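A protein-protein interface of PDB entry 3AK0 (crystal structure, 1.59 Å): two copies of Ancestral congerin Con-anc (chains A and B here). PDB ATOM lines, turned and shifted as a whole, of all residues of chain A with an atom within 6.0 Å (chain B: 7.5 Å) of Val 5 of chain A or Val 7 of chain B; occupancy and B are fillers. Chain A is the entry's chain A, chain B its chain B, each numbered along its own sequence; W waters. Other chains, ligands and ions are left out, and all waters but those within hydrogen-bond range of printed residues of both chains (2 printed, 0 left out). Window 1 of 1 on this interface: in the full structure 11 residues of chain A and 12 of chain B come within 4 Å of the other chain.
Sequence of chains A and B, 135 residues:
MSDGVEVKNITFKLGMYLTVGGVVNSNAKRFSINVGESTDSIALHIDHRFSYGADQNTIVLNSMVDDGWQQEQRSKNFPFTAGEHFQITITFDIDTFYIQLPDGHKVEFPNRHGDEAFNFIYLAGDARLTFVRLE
Of the 10 printed residues of chain A, 5 touch a printed residue of chain B.
Printed residues of chain A that touch a printed residue of chain B: Gly 4, Val 5, Glu 6, Val 7 and Lys 8.
Hydrophobic or aromatic side chains of chain B within 4 Å of the printed part of chain A: Val 5, Val 7 and Ile 10.
Among the printed residues, 13 pairs touch across the chains.
Among the printed residues, no Asp or Glu carboxylate lies within 4 Å of a Lys or Arg side-chain nitrogen of the other chain.
Val 5 of chain A touches four residues of chain B.
Of the printed residues of chain B, Lys 8 of chain A touches Val 5 (3.4 Å) and Glu 6 (2.8 Å).
Of the printed residues of chain A, Val 5 of chain B touches Val 7 and Lys 8.
Of the printed residues of chain A, Glu 6 of chain B touches Glu 6, Val 7 and Lys 8.
Of chain A, only Val 5 (3.7 Å) and Glu 6 (3.4 Å) come within 4 Å of Val 7 of chain B.
Ile 121 of chain B touches none of the printed residues of chain A.
The nearest printed residue of chain A that does not touch Val 5 of chain B is Glu 6 of chain A (7.2 Å).
O of Glu 6 of chain A lies within hydrogen-bond range of N of Lys 8 of chain B.
The backbone NH of Lys 8 of chain A is in hydrogen-bond range of the backbone carbonyl oxygen of Glu 6 of chain B.
Val 5 of chain A touches Val 7 of chain B, and with the chains exchanged Val 7 of chain A touches Val 5 of chain B.
Glu 6 of chain A touches its own counterpart, Glu 6 of chain B.
Glu 6 of chain A touches Val 7 of chain B, and with the chains exchanged Val 7 of chain A touches Glu 6 of chain B.
Glu 6 of chain A touches Lys 8 of chain B, and with the chains exchanged Lys 8 of chain A touches Glu 6 of chain B.
9 positions are printed for both chains.
Of the 13 pairs that touch across the chains among the printed residues, 9 have their exchanged pair printed and touching as well.
N of Gly 4 of chain A lies within hydrogen-bond range of O of Leu 123 of chain A (2.9 Å).
The backbone carbonyl oxygen (O) of Val 5 of chain A is in hydrogen-bond range of the backbone NH (N) of Leu 123 of chain A (2.9 Å).
N of Val 7 of chain A sits at hydrogen-bond distance from O of Ile 121 of chain A, at 2.8 Å.
The backbone NH of Leu 123 of chain B sits at hydrogen-bond distance from the backbone carbonyl oxygen of Val 5 of chain B (3.0 Å).
The backbone NH (N) of Val 7 of chain B sits at hydrogen-bond distance from the backbone carbonyl oxygen (O) of Ile 121 of chain B (2.8 Å).
The backbone carbonyl oxygen (O) of Asn 119 of chain B sits at hydrogen-bond distance from the backbone NH (N) of Asn 9 of chain B, 3.1 Å away.
Gly 4 of chain A touches Asn 9 of chain B.
Val 7 of chain B touches Val 5 of chain A (CG1 to CG2, 3.7 Å).
CA of Val 5 of chain A touches O of Lys 8 of chain B, at 3.4 Å.
O of Asn 9 of chain B touches N of Val 5 of chain A, 3.8 Å away.
Val 5 of chain A touches Ile 10 of chain B (CG2 to CG2, 3.5 Å).
O of Glu 6 of chain B touches O of Glu 6 of chain A, 3.5 Å away.
O of Glu 6 of chain A touches CA of Val 7 of chain B, at 3.4 Å.
Asn 9 of chain B touches Glu 6 of chain A (OD1 to OE2, 3.6 Å).
CG1 of Val 5 of chain B touches CG1 of Val 7 of chain A, at 3.6 Å.
Val 5 of chain B touches Lys 8 of chain A (CA to O, 3.4 Å).
Water W2 lies within hydrogen-bond range of O of Leu 129 of chain A and O of Leu 134 of chain B.
Water W1 lies within hydrogen-bond range of O of Glu 6 of chain B (3.1 Å) and O of Glu 6 of chain A (3.5 Å).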
ATOM      1  N   GLY A   4      26.322   8.097 -19.819  1.00  0.00           N
ATOM      2  CA  GLY A   4      26.653   9.294 -19.043  1.00  0.00           C
ATOM      3  C   GLY A   4      25.481  10.257 -19.105  1.00  0.00           C
ATOM      4  O   GLY A   4      24.322   9.838 -19.170  1.00  0.00           O
ATOM      5  N   VAL A   5      25.823  11.528 -19.062  1.00  0.00           N
ATOM      6  CA  VAL A   5      24.832  12.590 -19.003  1.00  0.00           C
ATOM      7  C   VAL A   5      23.825  12.494 -20.160  1.00  0.00           C
ATOM      8  O   VAL A   5      24.223  12.239 -21.308  1.00  0.00           O
ATOM      9  CB  VAL A   5      25.536  13.967 -18.992  1.00  0.00           C
ATOM     10  CG1 VAL A   5      26.412  14.177 -20.256  1.00  0.00           C
ATOM     11  CG2 VAL A   5      24.553  15.074 -18.841  1.00  0.00           C
ATOM     12  N   GLU A   6      22.535  12.691 -19.853  1.00  0.00           N
ATOM     13  CA  GLU A   6      21.472  12.893 -20.850  1.00  0.00           C
ATOM     14  C   GLU A   6      20.920  14.282 -20.643  1.00  0.00           C
ATOM     15  O   GLU A   6      20.622  14.670 -19.509  1.00  0.00           O
ATOM     16  CB  GLU A   6      20.346  11.868 -20.672  1.00  0.00           C
ATOM     17  CG  GLU A   6      20.859  10.438 -20.845  1.00  0.00           C
ATOM     18  CD  GLU A   6      19.789   9.364 -20.760  1.00  0.00           C
ATOM     19  OE1 GLU A   6      18.594   9.679 -20.924  1.00  0.00           O
ATOM     20  OE2 GLU A   6      20.152   8.186 -20.529  1.00  0.00           O
ATOM     21  N   VAL A   7      20.773  15.031 -21.727  1.00  0.00           N
ATOM     22  CA  VAL A   7      20.205  16.361 -21.657  1.00  0.00           C
ATOM     23  C   VAL A   7      18.963  16.306 -22.522  1.00  0.00           C
ATOM     24  O   VAL A   7      19.052  16.128 -23.720  1.00  0.00           O
ATOM     25  CB  VAL A   7      21.173  17.444 -22.182  1.00  0.00           C
ATOM     26  CG1 VAL A   7      20.532  18.862 -21.945  1.00  0.00           C
ATOM     27  CG2 VAL A   7      22.521  17.353 -21.479  1.00  0.00           C
ATOM     28  N   LYS A   8      17.816  16.445 -21.876  1.00  0.00           N
ATOM     29  CA  LYS A   8      16.528  16.286 -22.511  1.00  0.00           C
ATOM     30  C   LYS A   8      15.849  17.648 -22.668  1.00  0.00           C
ATOM     31  O   LYS A   8      15.972  18.518 -21.806  1.00  0.00           O
ATOM     32  CB  LYS A   8      15.698  15.338 -21.641  1.00  0.00           C
ATOM     33  CG  LYS A   8      14.332  14.994 -22.147  1.00  0.00           C
ATOM     34  CD  LYS A   8      13.591  14.233 -21.079  1.00  0.00           C
ATOM     35  CE  LYS A   8      12.171  13.940 -21.500  1.00  0.00           C
ATOM     36  NZ  LYS A   8      11.427  13.228 -20.432  1.00  0.00           N
ATOM     37  N   ILE A 121      20.623  15.474 -26.186  1.00  0.00           N
ATOM     38  CA  ILE A 121      22.059  15.144 -26.321  1.00  0.00           C
ATOM     39  C   ILE A 121      22.393  14.121 -25.231  1.00  0.00           C
ATOM     40  O   ILE A 121      21.835  14.157 -24.140  1.00  0.00           O
ATOM     41  CB  ILE A 121      22.957  16.410 -26.096  1.00  0.00           C
ATOM     42  CG1 ILE A 121      22.543  17.547 -27.030  1.00  0.00           C
ATOM     43  CG2 ILE A 121      24.496  16.072 -26.203  1.00  0.00           C
ATOM     44  CD1 ILE A 121      22.832  18.924 -26.456  1.00  0.00           C
ATOM     45  N   TYR A 122      23.311  13.196 -25.515  1.00  0.00           N
ATOM     46  CA  TYR A 122      23.853  12.427 -24.411  1.00  0.00           C
ATOM     47  C   TYR A 122      25.268  11.995 -24.671  1.00  0.00           C
ATOM     48  O   TYR A 122      25.701  11.901 -25.827  1.00  0.00           O
ATOM     49  CB  TYR A 122      22.946  11.243 -24.035  1.00  0.00           C
ATOM     50  CG  TYR A 122      23.075   9.986 -24.859  1.00  0.00           C
ATOM     51  CD1 TYR A 122      23.728   8.875 -24.343  1.00  0.00           C
ATOM     52  CD2 TYR A 122      22.475   9.885 -26.117  1.00  0.00           C
ATOM     53  CE1 TYR A 122      23.825   7.692 -25.061  1.00  0.00           C
ATOM     54  CE2 TYR A 122      22.561   8.707 -26.839  1.00  0.00           C
ATOM     55  CZ  TYR A 122      23.250   7.615 -26.306  1.00  0.00           C
ATOM     56  OH  TYR A 122      23.380   6.421 -27.009  1.00  0.00           O
ATOM     57  N   LEU A 123      25.995  11.731 -23.584  1.00  0.00           N
ATOM     58  CA  LEU A 123      27.350  11.236 -23.703  1.00  0.00           C
ATOM     59  C   LEU A 123      27.317   9.773 -23.290  1.00  0.00           C
ATOM     60  O   LEU A 123      26.593   9.385 -22.363  1.00  0.00           O
ATOM     61  CB  LEU A 123      28.313  12.047 -22.801  1.00  0.00           C
ATOM     62  CG  LEU A 123      29.805  11.663 -22.791  1.00  0.00           C
ATOM     63  CD1 LEU A 123      30.574  12.866 -22.345  1.00  0.00           C
ATOM     64  CD2 LEU A 123      30.074  10.447 -21.878  1.00  0.00           C
ATOM     65  N   ALA A 124      28.055   8.951 -24.012  1.00  0.00           N
ATOM     66  CA  ALA A 124      28.271   7.572 -23.566  1.00  0.00           C
ATOM     67  C   ALA A 124      29.747   7.290 -23.454  1.00  0.00           C
ATOM     68  O   ALA A 124      30.552   7.816 -24.225  1.00  0.00           O
ATOM     69  CB  ALA A 124      27.609   6.543 -24.530  1.00  0.00           C
ATOM     70  N   LEU A 129      31.356  14.661 -18.911  1.00  0.00           N
ATOM     71  CA  LEU A 129      30.955  16.004 -19.321  1.00  0.00           C
ATOM     72  C   LEU A 129      31.153  17.013 -18.205  1.00  0.00           C
ATOM     73  O   LEU A 129      30.795  16.762 -17.037  1.00  0.00           O
ATOM     74  CB  LEU A 129      29.497  15.978 -19.772  1.00  0.00           C
ATOM     75  CG  LEU A 129      29.057  17.238 -20.497  1.00  0.00           C
ATOM     76  CD1 LEU A 129      28.368  16.894 -21.800  1.00  0.00           C
ATOM     77  CD2 LEU A 129      28.141  18.037 -19.560  1.00  0.00           C
ATOM     78  N   GLY B   4      10.837  22.258 -19.504  1.00  0.00           N
ATOM     79  CA  GLY B   4      12.224  22.835 -19.604  1.00  0.00           C
ATOM     80  C   GLY B   4      13.339  21.795 -19.771  1.00  0.00           C
ATOM     81  O   GLY B   4      13.070  20.605 -19.901  1.00  0.00           O
ATOM     82  N   VAL B   5      14.589  22.257 -19.724  1.00  0.00           N
ATOM     83  CA  VAL B   5      15.753  21.401 -20.022  1.00  0.00           C
ATOM     84  C   VAL B   5      16.046  20.540 -18.802  1.00  0.00           C
ATOM     85  O   VAL B   5      16.139  21.069 -17.690  1.00  0.00           O
ATOM     86  CB  VAL B   5      16.986  22.232 -20.372  1.00  0.00           C
ATOM     87  CG1 VAL B   5      18.202  21.321 -20.685  1.00  0.00           C
ATOM     88  CG2 VAL B   5      16.705  23.161 -21.532  1.00  0.00           C
ATOM     89  N   GLU B   6      16.172  19.225 -19.001  1.00  0.00           N
ATOM     90  CA  GLU B   6      16.473  18.307 -17.886  1.00  0.00           C
ATOM     91  C   GLU B   6      17.819  17.637 -18.104  1.00  0.00           C
ATOM     92  O   GLU B   6      18.000  16.984 -19.130  1.00  0.00           O
ATOM     93  CB  GLU B   6      15.413  17.213 -17.796  1.00  0.00           C
ATOM     94  CG  GLU B   6      13.984  17.706 -17.580  1.00  0.00           C
ATOM     95  CD  GLU B   6      12.966  16.580 -17.511  1.00  0.00           C
ATOM     96  OE1 GLU B   6      13.330  15.440 -17.149  1.00  0.00           O
ATOM     97  OE2 GLU B   6      11.772  16.850 -17.782  1.00  0.00           O
ATOM     98  N   VAL B   7      18.730  17.758 -17.139  1.00  0.00           N
ATOM     99  CA  VAL B   7      20.044  17.137 -17.236  1.00  0.00           C
ATOM    100  C   VAL B   7      20.027  16.005 -16.215  1.00  0.00           C
ATOM    101  O   VAL B   7      19.809  16.256 -15.017  1.00  0.00           O
ATOM    102  CB  VAL B   7      21.170  18.135 -16.851  1.00  0.00           C
ATOM    103  CG1 VAL B   7      22.554  17.476 -16.923  1.00  0.00           C
ATOM    104  CG2 VAL B   7      21.139  19.405 -17.701  1.00  0.00           C
ATOM    105  N   LYS B   8      20.216  14.768 -16.672  1.00  0.00           N
ATOM    106  CA  LYS B   8      20.195  13.623 -15.756  1.00  0.00           C
ATOM    107  C   LYS B   8      21.456  12.796 -15.878  1.00  0.00           C
ATOM    108  O   LYS B   8      22.236  12.957 -16.830  1.00  0.00           O
ATOM    109  CB  LYS B   8      18.940  12.743 -15.945  1.00  0.00           C
ATOM    110  CG  LYS B   8      19.020  11.635 -16.966  1.00  0.00           C
ATOM    111  CD  LYS B   8      17.784  10.738 -16.803  1.00  0.00           C
ATOM    112  CE  LYS B   8      17.687   9.635 -17.839  1.00  0.00           C
ATOM    113  NZ  LYS B   8      16.539   8.751 -17.486  1.00  0.00           N
ATOM    114  N   ASN B   9      21.679  11.930 -14.898  1.00  0.00           N
ATOM    115  CA  ASN B   9      22.848  11.085 -14.856  1.00  0.00           C
ATOM    116  C   ASN B   9      24.128  11.887 -14.759  1.00  0.00           C
ATOM    117  O   ASN B   9      25.141  11.507 -15.345  1.00  0.00           O
ATOM    118  CB  ASN B   9      22.948  10.182 -16.112  1.00  0.00           C
ATOM    119  CG  ASN B   9      21.954   9.056 -16.115  1.00  0.00           C
ATOM    120  OD1 ASN B   9      21.592   8.559 -17.198  1.00  0.00           O
ATOM    121  ND2 ASN B   9      21.478   8.651 -14.937  1.00  0.00           N
ATOM    122  N   ILE B  10      24.080  13.033 -14.095  1.00  0.00           N
ATOM    123  CA  ILE B  10      25.305  13.720 -13.751  1.00  0.00           C
ATOM    124  C   ILE B  10      25.644  13.437 -12.285  1.00  0.00           C
ATOM    125  O   ILE B  10      24.811  12.926 -11.542  1.00  0.00           O
ATOM    126  CB  ILE B  10      25.248  15.253 -13.966  1.00  0.00           C
ATOM    127  CG1 ILE B  10      23.988  15.866 -13.362  1.00  0.00           C
ATOM    128  CG2 ILE B  10      25.387  15.612 -15.437  1.00  0.00           C
ATOM    129  CD1 ILE B  10      24.156  16.113 -11.877  1.00  0.00           C
ATOM    130  N   THR B  11      26.874  13.754 -11.892  1.00  0.00           N
ATOM    131  CA  THR B  11      27.276  13.650 -10.481  1.00  0.00           C
ATOM    132  C   THR B  11      27.623  15.033  -9.943  1.00  0.00           C
ATOM    133  O   THR B  11      28.683  15.591 -10.287  1.00  0.00           O
ATOM    134  CB  THR B  11      28.466  12.688 -10.286  1.00  0.00           C
ATOM    135  OG1 THR B  11      28.126  11.388 -10.787  1.00  0.00           O
ATOM    136  CG2 THR B  11      28.835  12.588  -8.810  1.00  0.00           C
ATOM    137  N   LEU B  18      28.331  24.078  -9.449  1.00  0.00           N
ATOM    138  CA  LEU B  18      27.475  24.048 -10.624  1.00  0.00           C
ATOM    139  C   LEU B  18      27.167  25.490 -10.986  1.00  0.00           C
ATOM    140  O   LEU B  18      26.719  26.261 -10.133  1.00  0.00           O
ATOM    141  CB  LEU B  18      26.167  23.322 -10.288  1.00  0.00           C
ATOM    142  CG  LEU B  18      25.011  23.503 -11.263  1.00  0.00           C
ATOM    143  CD1 LEU B  18      25.411  22.851 -12.599  1.00  0.00           C
ATOM    144  CD2 LEU B  18      23.726  22.886 -10.708  1.00  0.00           C
ATOM    145  N   ASN B  34      16.467  23.899 -10.674  1.00  0.00           N
ATOM    146  CA  ASN B  34      16.113  22.816  -9.767  1.00  0.00           C
ATOM    147  C   ASN B  34      17.203  21.772  -9.710  1.00  0.00           C
ATOM    148  O   ASN B  34      17.667  21.331 -10.759  1.00  0.00           O
ATOM    149  CB  ASN B  34      14.859  22.125 -10.282  1.00  0.00           C
ATOM    150  CG  ASN B  34      13.668  23.053 -10.352  1.00  0.00           C
ATOM    151  OD1 ASN B  34      12.877  23.135  -9.410  1.00  0.00           O
ATOM    152  ND2 ASN B  34      13.512  23.739 -11.483  1.00  0.00           N
ATOM    153  N   GLY B  36      18.260  18.028  -7.817  1.00  0.00           N
ATOM    154  CA  GLY B  36      17.681  16.902  -7.049  1.00  0.00           C
ATOM    155  C   GLY B  36      17.942  15.567  -7.717  1.00  0.00           C
ATOM    156  O   GLY B  36      19.059  15.291  -8.164  1.00  0.00           O
ATOM    157  N   GLU B  37      16.870  14.768  -7.795  1.00  0.00           N
ATOM    158  CA  GLU B  37      16.878  13.418  -8.367  1.00  0.00           C
ATOM    159  C   GLU B  37      15.979  13.258  -9.589  1.00  0.00           C
ATOM    160  O   GLU B  37      16.280  12.448 -10.473  1.00  0.00           O
ATOM    161  CB  GLU B  37      16.445  12.441  -7.292  1.00  0.00           C
ATOM    162  CG  GLU B  37      17.410  12.460  -6.143  1.00  0.00           C
ATOM    163  CD  GLU B  37      17.625  11.106  -5.522  1.00  0.00           C
ATOM    164  OE1 GLU B  37      18.735  10.902  -4.994  1.00  0.00           O
ATOM    165  OE2 GLU B  37      16.716  10.250  -5.574  1.00  0.00           O
ATOM    166  N   ASN B 119      21.790  14.030  -8.902  1.00  0.00           N
ATOM    167  CA  ASN B 119      21.944  13.489 -10.246  1.00  0.00           C
ATOM    168  C   ASN B 119      21.125  14.217 -11.297  1.00  0.00           C
ATOM    169  O   ASN B 119      21.197  13.863 -12.477  1.00  0.00           O
ATOM    170  CB  ASN B 119      21.557  11.999 -10.284  1.00  0.00           C
ATOM    171  CG  ASN B 119      20.109  11.777  -9.894  1.00  0.00           C
ATOM    172  OD1 ASN B 119      19.246  11.562 -10.747  1.00  0.00           O
ATOM    173  ND2 ASN B 119      19.830  11.862  -8.609  1.00  0.00           N
ATOM    174  N   PHE B 120      20.367  15.233 -10.889  1.00  0.00           N
ATOM    175  CA  PHE B 120      19.354  15.818 -11.775  1.00  0.00           C
ATOM    176  C   PHE B 120      19.341  17.321 -11.631  1.00  0.00           C
ATOM    177  O   PHE B 120      19.336  17.841 -10.507  1.00  0.00           O
ATOM    178  CB  PHE B 120      17.990  15.234 -11.394  1.00  0.00           C
ATOM    179  CG  PHE B 120      16.861  15.640 -12.289  1.00  0.00           C
ATOM    180  CD1 PHE B 120      16.756  15.120 -13.600  1.00  0.00           C
ATOM    181  CD2 PHE B 120      15.899  16.536 -11.825  1.00  0.00           C
ATOM    182  CE1 PHE B 120      15.669  15.493 -14.424  1.00  0.00           C
ATOM    183  CE2 PHE B 120      14.814  16.915 -12.646  1.00  0.00           C
ATOM    184  CZ  PHE B 120      14.719  16.389 -13.936  1.00  0.00           C
ATOM    185  N   ILE B 121      19.393  18.012 -12.760  1.00  0.00           N
ATOM    186  CA  ILE B 121      19.362  19.476 -12.797  1.00  0.00           C
ATOM    187  C   ILE B 121      18.304  19.862 -13.817  1.00  0.00           C
ATOM    188  O   ILE B 121      18.259  19.274 -14.886  1.00  0.00           O
ATOM    189  CB  ILE B 121      20.735  20.075 -13.191  1.00  0.00           C
ATOM    190  CG1 ILE B 121      21.822  19.673 -12.198  1.00  0.00           C
ATOM    191  CG2 ILE B 121      20.656  21.625 -13.285  1.00  0.00           C
ATOM    192  CD1 ILE B 121      23.237  19.676 -12.821  1.00  0.00           C
ATOM    193  N   TYR B 122      17.453  20.841 -13.503  1.00  0.00           N
ATOM    194  CA  TYR B 122      16.312  21.135 -14.370  1.00  0.00           C
ATOM    195  C   TYR B 122      16.037  22.633 -14.358  1.00  0.00           C
ATOM    196  O   TYR B 122      15.935  23.227 -13.287  1.00  0.00           O
ATOM    197  CB  TYR B 122      15.123  20.349 -13.816  1.00  0.00           C
ATOM    198  CG  TYR B 122      13.722  20.634 -14.291  1.00  0.00           C
ATOM    199  CD1 TYR B 122      13.401  20.666 -15.656  1.00  0.00           C
ATOM    200  CD2 TYR B 122      12.687  20.756 -13.375  1.00  0.00           C
ATOM    201  CE1 TYR B 122      12.088  20.890 -16.072  1.00  0.00           C
ATOM    202  CE2 TYR B 122      11.388  20.965 -13.773  1.00  0.00           C
ATOM    203  CZ  TYR B 122      11.087  21.022 -15.121  1.00  0.00           C
ATOM    204  OH  TYR B 122       9.788  21.214 -15.508  1.00  0.00           O
ATOM    205  N   LEU B 123      15.978  23.229 -15.553  1.00  0.00           N
ATOM    206  CA  LEU B 123      15.653  24.642 -15.727  1.00  0.00           C
ATOM    207  C   LEU B 123      14.273  24.714 -16.318  1.00  0.00           C
ATOM    208  O   LEU B 123      14.041  24.155 -17.398  1.00  0.00           O
ATOM    209  CB  LEU B 123      16.643  25.303 -16.682  1.00  0.00           C
ATOM    210  CG  LEU B 123      16.504  26.794 -17.017  1.00  0.00           C
ATOM    211  CD1 LEU B 123      16.757  27.683 -15.829  1.00  0.00           C
ATOM    212  CD2 LEU B 123      17.454  27.192 -18.171  1.00  0.00           C
ATOM    213  N   LEU B 129      18.221  28.400 -21.644  1.00  0.00           N
ATOM    214  CA  LEU B 129      19.541  27.971 -21.197  1.00  0.00           C
ATOM    215  C   LEU B 129      20.623  28.443 -22.161  1.00  0.00           C
ATOM    216  O   LEU B 129      20.472  28.321 -23.383  1.00  0.00           O
ATOM    217  CB  LEU B 129      19.619  26.433 -21.123  1.00  0.00           C
ATOM    218  CG  LEU B 129      20.931  25.835 -20.597  1.00  0.00           C
ATOM    219  CD1 LEU B 129      21.061  26.112 -19.105  1.00  0.00           C
ATOM    220  CD2 LEU B 129      21.005  24.327 -20.882  1.00  0.00           C
ATOM    221  N   VAL B 132      25.678  25.162 -19.015  1.00  0.00           N
ATOM    222  CA  VAL B 132      25.828  24.474 -17.720  1.00  0.00           C
ATOM    223  C   VAL B 132      27.289  24.084 -17.591  1.00  0.00           C
ATOM    224  O   VAL B 132      27.867  23.530 -18.539  1.00  0.00           O
ATOM    225  CB  VAL B 132      24.980  23.185 -17.662  1.00  0.00           C
ATOM    226  CG1 VAL B 132      25.324  22.321 -16.412  1.00  0.00           C
ATOM    227  CG2 VAL B 132      23.502  23.518 -17.737  1.00  0.00           C
ATOM    228  N   LEU B 134      29.928  22.209 -14.657  1.00  0.00           N
ATOM    229  CA  LEU B 134      29.922  21.419 -13.436  1.00  0.00           C
ATOM    230  C   LEU B 134      31.272  20.754 -13.279  1.00  0.00           C
ATOM    231  O   LEU B 134      31.667  19.952 -14.124  1.00  0.00           O
ATOM    232  CB  LEU B 134      28.802  20.350 -13.574  1.00  0.00           C
ATOM    233  CG  LEU B 134      28.496  19.272 -12.531  1.00  0.00           C
ATOM    234  CD1 LEU B 134      28.075  19.899 -11.199  1.00  0.00           C
ATOM    235  CD2 LEU B 134      27.415  18.318 -13.000  1.00  0.00           C
HETATM  236  O   HOH W   1      17.276  13.966 -18.932  1.00  0.00           O
HETATM  237  O   HOH W   2      31.048  17.172 -14.466  1.00  0.00           O
